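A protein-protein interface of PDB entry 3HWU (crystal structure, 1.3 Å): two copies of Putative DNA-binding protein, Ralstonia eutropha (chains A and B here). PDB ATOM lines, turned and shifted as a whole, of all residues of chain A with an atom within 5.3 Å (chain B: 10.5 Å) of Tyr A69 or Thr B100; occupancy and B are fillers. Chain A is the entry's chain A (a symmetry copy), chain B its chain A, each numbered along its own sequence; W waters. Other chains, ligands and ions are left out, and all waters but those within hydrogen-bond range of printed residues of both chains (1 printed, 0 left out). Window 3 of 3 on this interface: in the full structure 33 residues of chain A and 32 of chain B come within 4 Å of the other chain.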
ATOM      1  N   SER A  50      21.801 -20.708  11.141  1.00  0.00           N
ATOM      2  CA  SER A  50      22.110 -21.883  10.332  1.00  0.00           C
ATOM      3  C   SER A  50      20.932 -22.862  10.294  1.00  0.00           C
ATOM      4  O   SER A  50      20.697 -23.527   9.277  1.00  0.00           O
ATOM      5  CB  SER A  50      23.344 -22.584  10.848  1.00  0.00           C
ATOM      6  OG  SER A  50      23.241 -22.884  12.223  1.00  0.00           O
ATOM      7  N   GLU A  51      20.174 -22.925  11.379  1.00  0.00           N
ATOM      8  CA  GLU A  51      18.931 -23.667  11.329  1.00  0.00           C
ATOM      9  C   GLU A  51      17.956 -23.102  12.333  1.00  0.00           C
ATOM     10  O   GLU A  51      18.352 -22.610  13.381  1.00  0.00           O
ATOM     11  CB  GLU A  51      19.142 -25.137  11.567  1.00  0.00           C
ATOM     12  CG  GLU A  51      19.862 -25.421  12.799  1.00  0.00           C
ATOM     13  CD  GLU A  51      20.031 -26.919  13.028  1.00  0.00           C
ATOM     14  OE1 GLU A  51      19.104 -27.547  13.580  1.00  0.00           O
ATOM     15  OE2 GLU A  51      21.093 -27.444  12.651  1.00  0.00           O
ATOM     16  N   ALA A  52      16.688 -23.160  11.950  1.00  0.00           N
ATOM     17  CA  ALA A  52      15.577 -22.740  12.778  1.00  0.00           C
ATOM     18  C   ALA A  52      14.489 -23.789  12.583  1.00  0.00           C
ATOM     19  O   ALA A  52      14.042 -24.018  11.466  1.00  0.00           O
ATOM     20  CB  ALA A  52      15.101 -21.355  12.401  1.00  0.00           C
ATOM     21  N   THR A  53      14.012 -24.347  13.683  1.00  0.00           N
ATOM     22  CA  THR A  53      12.975 -25.388  13.690  1.00  0.00           C
ATOM     23  C   THR A  53      11.739 -24.869  14.403  1.00  0.00           C
ATOM     24  O   THR A  53      11.815 -24.419  15.537  1.00  0.00           O
ATOM     25  CB  THR A  53      13.487 -26.678  14.338  1.00  0.00           C
ATOM     26  OG1 THR A  53      14.660 -27.120  13.644  1.00  0.00           O
ATOM     27  CG2 THR A  53      12.426 -27.779  14.344  1.00  0.00           C
ATOM     28  N   PHE A  54      10.615 -24.938  13.699  1.00  0.00           N
ATOM     29  CA  PHE A  54       9.323 -24.536  14.191  1.00  0.00           C
ATOM     30  C   PHE A  54       8.450 -25.765  14.386  1.00  0.00           C
ATOM     31  O   PHE A  54       8.705 -26.831  13.825  1.00  0.00           O
ATOM     32  CB  PHE A  54       8.693 -23.609  13.154  1.00  0.00           C
ATOM     33  CG  PHE A  54       9.510 -22.359  12.932  1.00  0.00           C
ATOM     34  CD1 PHE A  54       9.307 -21.254  13.742  1.00  0.00           C
ATOM     35  CD2 PHE A  54      10.516 -22.314  11.974  1.00  0.00           C
ATOM     36  CE1 PHE A  54      10.040 -20.121  13.571  1.00  0.00           C
ATOM     37  CE2 PHE A  54      11.261 -21.151  11.816  1.00  0.00           C
ATOM     38  CZ  PHE A  54      11.016 -20.065  12.635  1.00  0.00           C
ATOM     39  N   LYS A  67       9.167 -28.365  11.387  1.00  0.00           N
ATOM     40  CA  LYS A  67       9.757 -27.957  10.108  1.00  0.00           C
ATOM     41  C   LYS A  67      11.036 -27.175  10.351  1.00  0.00           C
ATOM     42  O   LYS A  67      11.061 -26.251  11.170  1.00  0.00           O
ATOM     43  CB  LYS A  67       8.796 -27.113   9.276  1.00  0.00           C
ATOM     44  CG  LYS A  67       9.344 -26.777   7.910  1.00  0.00           C
ATOM     45  CD  LYS A  67       8.294 -26.397   6.915  1.00  0.00           C
ATOM     46  CE  LYS A  67       8.876 -26.071   5.580  1.00  0.00           C
ATOM     47  N   THR A  68      12.078 -27.543   9.609  1.00  0.00           N
ATOM     48  CA  THR A  68      13.374 -26.899   9.761  1.00  0.00           C
ATOM     49  C   THR A  68      13.751 -26.107   8.526  1.00  0.00           C
ATOM     50  O   THR A  68      13.633 -26.589   7.359  1.00  0.00           O
ATOM     51  CB  THR A  68      14.470 -27.935  10.050  1.00  0.00           C
ATOM     52  OG1 THR A  68      14.190 -28.562  11.302  1.00  0.00           O
ATOM     53  CG2 THR A  68      15.859 -27.287  10.151  1.00  0.00           C
ATOM     54  N   TYR A  69      14.195 -24.880   8.778  1.00  0.00           N
ATOM     55  CA  TYR A  69      14.751 -24.001   7.765  1.00  0.00           C
ATOM     56  C   TYR A  69      16.226 -23.809   8.013  1.00  0.00           C
ATOM     57  O   TYR A  69      16.657 -23.751   9.138  1.00  0.00           O
ATOM     58  CB  TYR A  69      14.044 -22.641   7.781  1.00  0.00           C
ATOM     59  CG  TYR A  69      12.587 -22.716   7.444  1.00  0.00           C
ATOM     60  CD1 TYR A  69      11.638 -23.020   8.398  1.00  0.00           C
ATOM     61  CD2 TYR A  69      12.147 -22.554   6.163  1.00  0.00           C
ATOM     62  CE1 TYR A  69      10.317 -23.111   8.043  1.00  0.00           C
ATOM     63  CE2 TYR A  69      10.837 -22.663   5.807  1.00  0.00           C
ATOM     64  CZ  TYR A  69       9.905 -22.937   6.754  1.00  0.00           C
ATOM     65  OH  TYR A  69       8.573 -23.023   6.365  1.00  0.00           O
ATOM     66  N   ARG A  70      17.002 -23.732   6.944  1.00  0.00           N
ATOM     67  CA  ARG A  70      18.439 -23.587   7.005  1.00  0.00           C
ATOM     68  C   ARG A  70      18.927 -22.284   6.404  1.00  0.00           C
ATOM     69  O   ARG A  70      18.426 -21.863   5.365  1.00  0.00           O
ATOM     70  CB  ARG A  70      19.158 -24.775   6.288  1.00  0.00           C
ATOM     71  CG  ARG A  70      18.729 -26.111   6.855  1.00  0.00           C
ATOM     72  CD  ARG A  70      19.393 -27.251   6.099  1.00  0.00           C
ATOM     73  NE  ARG A  70      18.993 -28.552   6.609  1.00  0.00           N
ATOM     74  CZ  ARG A  70      19.482 -29.062   7.733  1.00  0.00           C
ATOM     75  NH1 ARG A  70      20.324 -28.364   8.464  1.00  0.00           N
ATOM     76  NH2 ARG A  70      19.138 -30.283   8.124  1.00  0.00           N
ATOM     77  N   ASN A  71      19.956 -21.703   7.003  1.00  0.00           N
ATOM     78  CA  ASN A  71      20.627 -20.502   6.484  1.00  0.00           C
ATOM     79  C   ASN A  71      19.620 -19.387   6.144  1.00  0.00           C
ATOM     80  O   ASN A  71      19.433 -18.962   5.000  1.00  0.00           O
ATOM     81  CB  ASN A  71      21.547 -20.864   5.330  1.00  0.00           C
ATOM     82  CG  ASN A  71      22.786 -21.617   5.808  1.00  0.00           C
ATOM     83  OD1 ASN A  71      23.198 -21.487   6.942  1.00  0.00           O
ATOM     84  ND2 ASN A  71      23.385 -22.398   4.937  1.00  0.00           N
ATOM     85  N   VAL A  72      18.939 -18.934   7.199  1.00  0.00           N
ATOM     86  CA  VAL A  72      17.856 -17.969   7.093  1.00  0.00           C
ATOM     87  C   VAL A  72      18.088 -16.742   7.970  1.00  0.00           C
ATOM     88  O   VAL A  72      18.655 -16.831   9.061  1.00  0.00           O
ATOM     89  CB  VAL A  72      16.471 -18.561   7.453  1.00  0.00           C
ATOM     90  CG1 VAL A  72      15.985 -19.489   6.348  1.00  0.00           C
ATOM     91  CG2 VAL A  72      16.472 -19.235   8.806  1.00  0.00           C
ATOM     92  N   VAL A  96      11.282 -16.053   9.773  1.00  0.00           N
ATOM     93  CA  VAL A  96      12.541 -16.259   9.035  1.00  0.00           C
ATOM     94  C   VAL A  96      12.302 -16.082   7.547  1.00  0.00           C
ATOM     95  O   VAL A  96      11.192 -16.316   7.056  1.00  0.00           O
ATOM     96  CB  VAL A  96      13.212 -17.625   9.335  1.00  0.00           C
ATOM     97  CG1 VAL A  96      13.637 -17.718  10.818  1.00  0.00           C
ATOM     98  CG2 VAL A  96      12.325 -18.818   8.970  1.00  0.00           C
ATOM     99  N   ALA A 104       8.423 -17.172   6.778  1.00  0.00           N
ATOM    100  CA  ALA A 104       7.896 -18.392   7.368  1.00  0.00           C
ATOM    101  C   ALA A 104       8.192 -18.348   8.841  1.00  0.00           C
ATOM    102  O   ALA A 104       8.987 -17.512   9.298  1.00  0.00           O
ATOM    103  CB  ALA A 104       8.587 -19.637   6.735  1.00  0.00           C
ATOM    104  N   GLY A 105       7.527 -19.200   9.612  1.00  0.00           N
ATOM    105  CA  GLY A 105       7.850 -19.300  11.012  1.00  0.00           C
ATOM    106  C   GLY A 105       6.683 -19.762  11.853  1.00  0.00           C
ATOM    107  O   GLY A 105       5.891 -20.614  11.407  1.00  0.00           O
ATOM    108  N   TYR B  69      -7.774 -15.281   8.651  1.00  0.00           N
ATOM    109  CA  TYR B  69      -7.072 -16.533   8.858  1.00  0.00           C
ATOM    110  C   TYR B  69      -7.578 -17.199  10.112  1.00  0.00           C
ATOM    111  O   TYR B  69      -7.896 -16.542  11.072  1.00  0.00           O
ATOM    112  CB  TYR B  69      -5.562 -16.293   8.977  1.00  0.00           C
ATOM    113  CG  TYR B  69      -4.944 -15.726   7.738  1.00  0.00           C
ATOM    114  CD1 TYR B  69      -4.958 -14.371   7.478  1.00  0.00           C
ATOM    115  CD2 TYR B  69      -4.401 -16.533   6.781  1.00  0.00           C
ATOM    116  CE1 TYR B  69      -4.409 -13.892   6.316  1.00  0.00           C
ATOM    117  CE2 TYR B  69      -3.874 -16.059   5.618  1.00  0.00           C
ATOM    118  CZ  TYR B  69      -3.867 -14.724   5.380  1.00  0.00           C
ATOM    119  OH  TYR B  69      -3.304 -14.268   4.194  1.00  0.00           O
ATOM    120  N   ARG B  70      -7.673 -18.519  10.086  1.00  0.00           N
ATOM    121  CA  ARG B  70      -8.176 -19.310  11.188  1.00  0.00           C
ATOM    122  C   ARG B  70      -7.134 -20.245  11.767  1.00  0.00           C
ATOM    123  O   ARG B  70      -6.375 -20.855  11.020  1.00  0.00           O
ATOM    124  CB  ARG B  70      -9.423 -20.146  10.759  1.00  0.00           C
ATOM    125  CG  ARG B  70     -10.515 -19.267  10.186  1.00  0.00           C
ATOM    126  CD  ARG B  70     -11.691 -20.111   9.720  1.00  0.00           C
ATOM    127  NE  ARG B  70     -12.754 -19.301   9.151  1.00  0.00           N
ATOM    128  CZ  ARG B  70     -13.600 -18.601   9.899  1.00  0.00           C
ATOM    129  NH1 ARG B  70     -13.463 -18.581  11.206  1.00  0.00           N
ATOM    130  NH2 ARG B  70     -14.598 -17.929   9.338  1.00  0.00           N
ATOM    131  N   ASN B  71      -7.160 -20.423  13.080  1.00  0.00           N
ATOM    132  CA  ASN B  71      -6.302 -21.383  13.788  1.00  0.00           C
ATOM    133  C   ASN B  71      -4.822 -21.228  13.388  1.00  0.00           C
ATOM    134  O   ASN B  71      -4.178 -22.105  12.802  1.00  0.00           O
ATOM    135  CB  ASN B  71      -6.833 -22.797  13.620  1.00  0.00           C
ATOM    136  CG  ASN B  71      -8.114 -23.018  14.420  1.00  0.00           C
ATOM    137  OD1 ASN B  71      -8.360 -22.352  15.403  1.00  0.00           O
ATOM    138  ND2 ASN B  71      -8.925 -23.964  14.002  1.00  0.00           N
ATOM    139  N   VAL B  72      -4.297 -20.043  13.707  1.00  0.00           N
ATOM    140  CA  VAL B  72      -2.955 -19.637  13.320  1.00  0.00           C
ATOM    141  C   VAL B  72      -2.110 -19.218  14.519  1.00  0.00           C
ATOM    142  O   VAL B  72      -2.611 -18.646  15.490  1.00  0.00           O
ATOM    143  CB  VAL B  72      -2.940 -18.478  12.294  1.00  0.00           C
ATOM    144  CG1 VAL B  72      -3.373 -18.974  10.922  1.00  0.00           C
ATOM    145  CG2 VAL B  72      -3.757 -17.292  12.758  1.00  0.00           C
ATOM    146  N   GLU B  73      -0.830 -19.551  14.471  1.00  0.00           N
ATOM    147  CA  GLU B  73       0.143 -18.971  15.410  1.00  0.00           C
ATOM    148  C   GLU B  73       0.405 -17.531  15.018  1.00  0.00           C
ATOM    149  O   GLU B  73       0.572 -17.243  13.838  1.00  0.00           O
ATOM    150  CB  GLU B  73       1.449 -19.761  15.389  1.00  0.00           C
ATOM    151  CG  GLU B  73       1.358 -21.174  16.033  1.00  0.00           C
ATOM    152  CD  GLU B  73       1.265 -21.165  17.553  1.00  0.00           C
ATOM    153  OE1 GLU B  73       1.086 -20.104  18.156  1.00  0.00           O
ATOM    154  OE2 GLU B  73       1.395 -22.263  18.151  1.00  0.00           O
ATOM    155  N   VAL B  96       1.153 -13.960  11.091  1.00  0.00           N
ATOM    156  CA  VAL B  96       0.546 -15.251  11.462  1.00  0.00           C
ATOM    157  C   VAL B  96       1.047 -16.343  10.537  1.00  0.00           C
ATOM    158  O   VAL B  96       1.399 -16.077   9.382  1.00  0.00           O
ATOM    159  CB  VAL B  96      -1.006 -15.212  11.494  1.00  0.00           C
ATOM    160  CG1 VAL B  96      -1.511 -14.241  12.584  1.00  0.00           C
ATOM    161  CG2 VAL B  96      -1.621 -14.846  10.141  1.00  0.00           C
ATOM    162  N   THR B  97       1.073 -17.561  11.053  1.00  0.00           N
ATOM    163  CA  THR B  97       1.523 -18.714  10.300  1.00  0.00           C
ATOM    164  C   THR B  97       0.634 -19.913  10.662  1.00  0.00           C
ATOM    165  O   THR B  97       0.063 -19.979  11.761  1.00  0.00           O
ATOM    166  CB  THR B  97       2.992 -19.078  10.616  1.00  0.00           C
ATOM    167  OG1 THR B  97       3.103 -19.462  11.991  1.00  0.00           O
ATOM    168  CG2 THR B  97       3.953 -17.900  10.330  1.00  0.00           C
ATOM    169  N   ASP B  98       0.557 -20.876   9.749  1.00  0.00           N
ATOM    170  CA  ASP B  98      -0.268 -22.066   9.963  1.00  0.00           C
ATOM    171  C   ASP B  98       0.587 -23.320   9.832  1.00  0.00           C
ATOM    172  O   ASP B  98       1.798 -23.293   9.992  1.00  0.00           O
ATOM    173  CB  ASP B  98      -1.444 -22.091   8.983  1.00  0.00           C
ATOM    174  CG  ASP B  98      -1.006 -22.284   7.537  1.00  0.00           C
ATOM    175  OD1 ASP B  98       0.216 -22.353   7.281  1.00  0.00           O
ATOM    176  OD2 ASP B  98      -1.922 -22.288   6.652  1.00  0.00           O
ATOM    177  N   GLY B  99      -0.048 -24.458   9.550  1.00  0.00           N
ATOM    178  CA  GLY B  99       0.689 -25.697   9.430  1.00  0.00           C
ATOM    179  C   GLY B  99       1.573 -25.813   8.199  1.00  0.00           C
ATOM    180  O   GLY B  99       2.335 -26.760   8.101  1.00  0.00           O
ATOM    181  N   THR B 100       1.513 -24.848   7.290  1.00  0.00           N
ATOM    182  CA  THR B 100       2.495 -24.750   6.206  1.00  0.00           C
ATOM    183  C   THR B 100       3.734 -23.950   6.639  1.00  0.00           C
ATOM    184  O   THR B 100       4.717 -23.910   5.902  1.00  0.00           O
ATOM    185  CB  THR B 100       1.945 -24.026   4.975  1.00  0.00           C
ATOM    186  OG1 THR B 100       1.805 -22.619   5.229  1.00  0.00           O
ATOM    187  CG2 THR B 100       0.649 -24.639   4.493  1.00  0.00           C
ATOM    188  N   PHE B 101       3.618 -23.265   7.775  1.00  0.00           N
ATOM    189  CA  PHE B 101       4.613 -22.320   8.306  1.00  0.00           C
ATOM    190  C   PHE B 101       4.804 -21.066   7.506  1.00  0.00           C
ATOM    191  O   PHE B 101       5.595 -20.189   7.858  1.00  0.00           O
ATOM    192  CB  PHE B 101       5.936 -23.018   8.621  1.00  0.00           C
ATOM    193  CG  PHE B 101       5.772 -24.216   9.516  1.00  0.00           C
ATOM    194  CD1 PHE B 101       5.826 -24.067  10.882  1.00  0.00           C
ATOM    195  CD2 PHE B 101       5.529 -25.489   9.002  1.00  0.00           C
ATOM    196  CE1 PHE B 101       5.663 -25.166  11.700  1.00  0.00           C
ATOM    197  CE2 PHE B 101       5.305 -26.586   9.839  1.00  0.00           C
ATOM    198  CZ  PHE B 101       5.406 -26.413  11.176  1.00  0.00           C
ATOM    199  N   GLN B 102       4.035 -20.875   6.451  1.00  0.00           N
ATOM    200  CA  GLN B 102       4.178 -19.662   5.632  1.00  0.00           C
ATOM    201  C   GLN B 102       3.544 -18.479   6.356  1.00  0.00           C
ATOM    202  O   GLN B 102       2.499 -18.612   7.028  1.00  0.00           O
ATOM    203  CB  GLN B 102       3.512 -19.817   4.273  1.00  0.00           C
ATOM    204  CG  GLN B 102       4.187 -20.862   3.414  1.00  0.00           C
ATOM    205  CD  GLN B 102       3.370 -21.296   2.196  1.00  0.00           C
ATOM    206  OE1 GLN B 102       2.449 -20.601   1.735  1.00  0.00           O
ATOM    207  NE2 GLN B 102       3.674 -22.482   1.712  1.00  0.00           N
ATOM    208  N   GLY B 103       4.214 -17.341   6.279  1.00  0.00           N
ATOM    209  CA  GLY B 103       3.735 -16.133   6.957  1.00  0.00           C
ATOM    210  C   GLY B 103       2.810 -15.234   6.187  1.00  0.00           C
ATOM    211  O   GLY B 103       2.946 -15.080   4.978  1.00  0.00           O
ATOM    212  N   ALA B 104       1.883 -14.610   6.915  1.00  0.00           N
ATOM    213  CA  ALA B 104       0.933 -13.671   6.338  1.00  0.00           C
ATOM    214  C   ALA B 104       0.605 -12.653   7.393  1.00  0.00           C
ATOM    215  O   ALA B 104       0.929 -12.845   8.576  1.00  0.00           O
ATOM    216  CB  ALA B 104      -0.367 -14.417   5.913  1.00  0.00           C
HETATM  217  O   HOH W   1       3.135 -22.126  12.178  1.00  0.00           O
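CB of Phe A54 touches CD1 of Phe B101, at 3.7 Å. Lys A67 touches Phe B101. Tyr A69 touches Thr B100. Tyr A69 touches Phe B101 (OH to CB, 3.5 Å). Ala A104 touches Phe B101. Gly B103 touches Ala A104 (N to CA, 3.98 Å).
The backbone carbonyl oxygen (O) of Gly A105 lies within hydrogen-bond range of the side-chain hydroxyl (OG1) of Thr B97 (3.1 Å). The backbone NH of Gly A105 is in hydrogen-bond range of the backbone carbonyl oxygen of Phe B101.
The backbone carbonyl oxygen (O) of Glu B73 sits at hydrogen-bond distance from the backbone NH (N) of Thr B97. The side-chain carboxylate (OD1) of Asp B98 lies within hydrogen-bond range of the side-chain hydroxyl (OG1) of Thr B100 (2.6 Å). The side-chain hydroxyl of Thr B100 is in hydrogen-bond range of the backbone NH of Gln B102 (3.1 Å). The backbone carbonyl oxygen (O) of Ala A52 sits at hydrogen-bond distance from the backbone NH (N) of Tyr A69, 2.8 Å away. The backbone carbonyl oxygen of Lys A67 is in hydrogen-bond range of the backbone NH of Phe A54 (2.9 Å). O of Ala A104 is in hydrogen-bond range of N of Val A96, 2.8 Å away.
Hydrophobic or aromatic side chains of chain A that line the printed part of chain B: Phe A54, Tyr A69 and Ala A104. Among the printed residues, no Asp or Glu carboxylate lies within 4 Å of a Lys or Arg side-chain nitrogen of the other chain.
6 positions are printed for both chains. Of the 8 pairs that touch across the chains among the printed residues, none has its exchanged pair printed and touching as well.
Water W1 lies within hydrogen-bond range of OG1 of Thr B97 (2.7 Å), O of Asp B98 (2.8 Å) and O of Gly A105 (3.2 Å).
Of the printed residues of chain A, Thr B100 touches Tyr A69 (3.98 Å). Ala A52 touches none of the printed residues of chain B. Lys A67 touches just one residue of chain B: Phe B101 (3.6 Å). Gly A105 touches two residues of chain B. Printed residues of chain A within 4 Å of Gly B103: Ala A104 (3.98 Å). Of the printed residues of chain A, Phe B101 touches Phe A54, Lys A67, Tyr A69, Ala A104 and Gly A105. Of the printed residues of chain B, Ala A104 touches Phe B101 and Gly B103. Of the printed residues of chain B, Phe A54 touches Phe B101. Val A96 touches none of the printed residues of chain B. Asp B98 touches none of the printed residues of chain A. The nearest printed residue of chain B that does not touch Tyr A69 is Gln B102 (5.0 Å). The nearest printed residue of chain A that does not touch Thr B100 is Lys A67 (4.5 Å). The nearest printed residue of chain A that does not touch Phe B101 is Thr A53 (6.7 Å).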
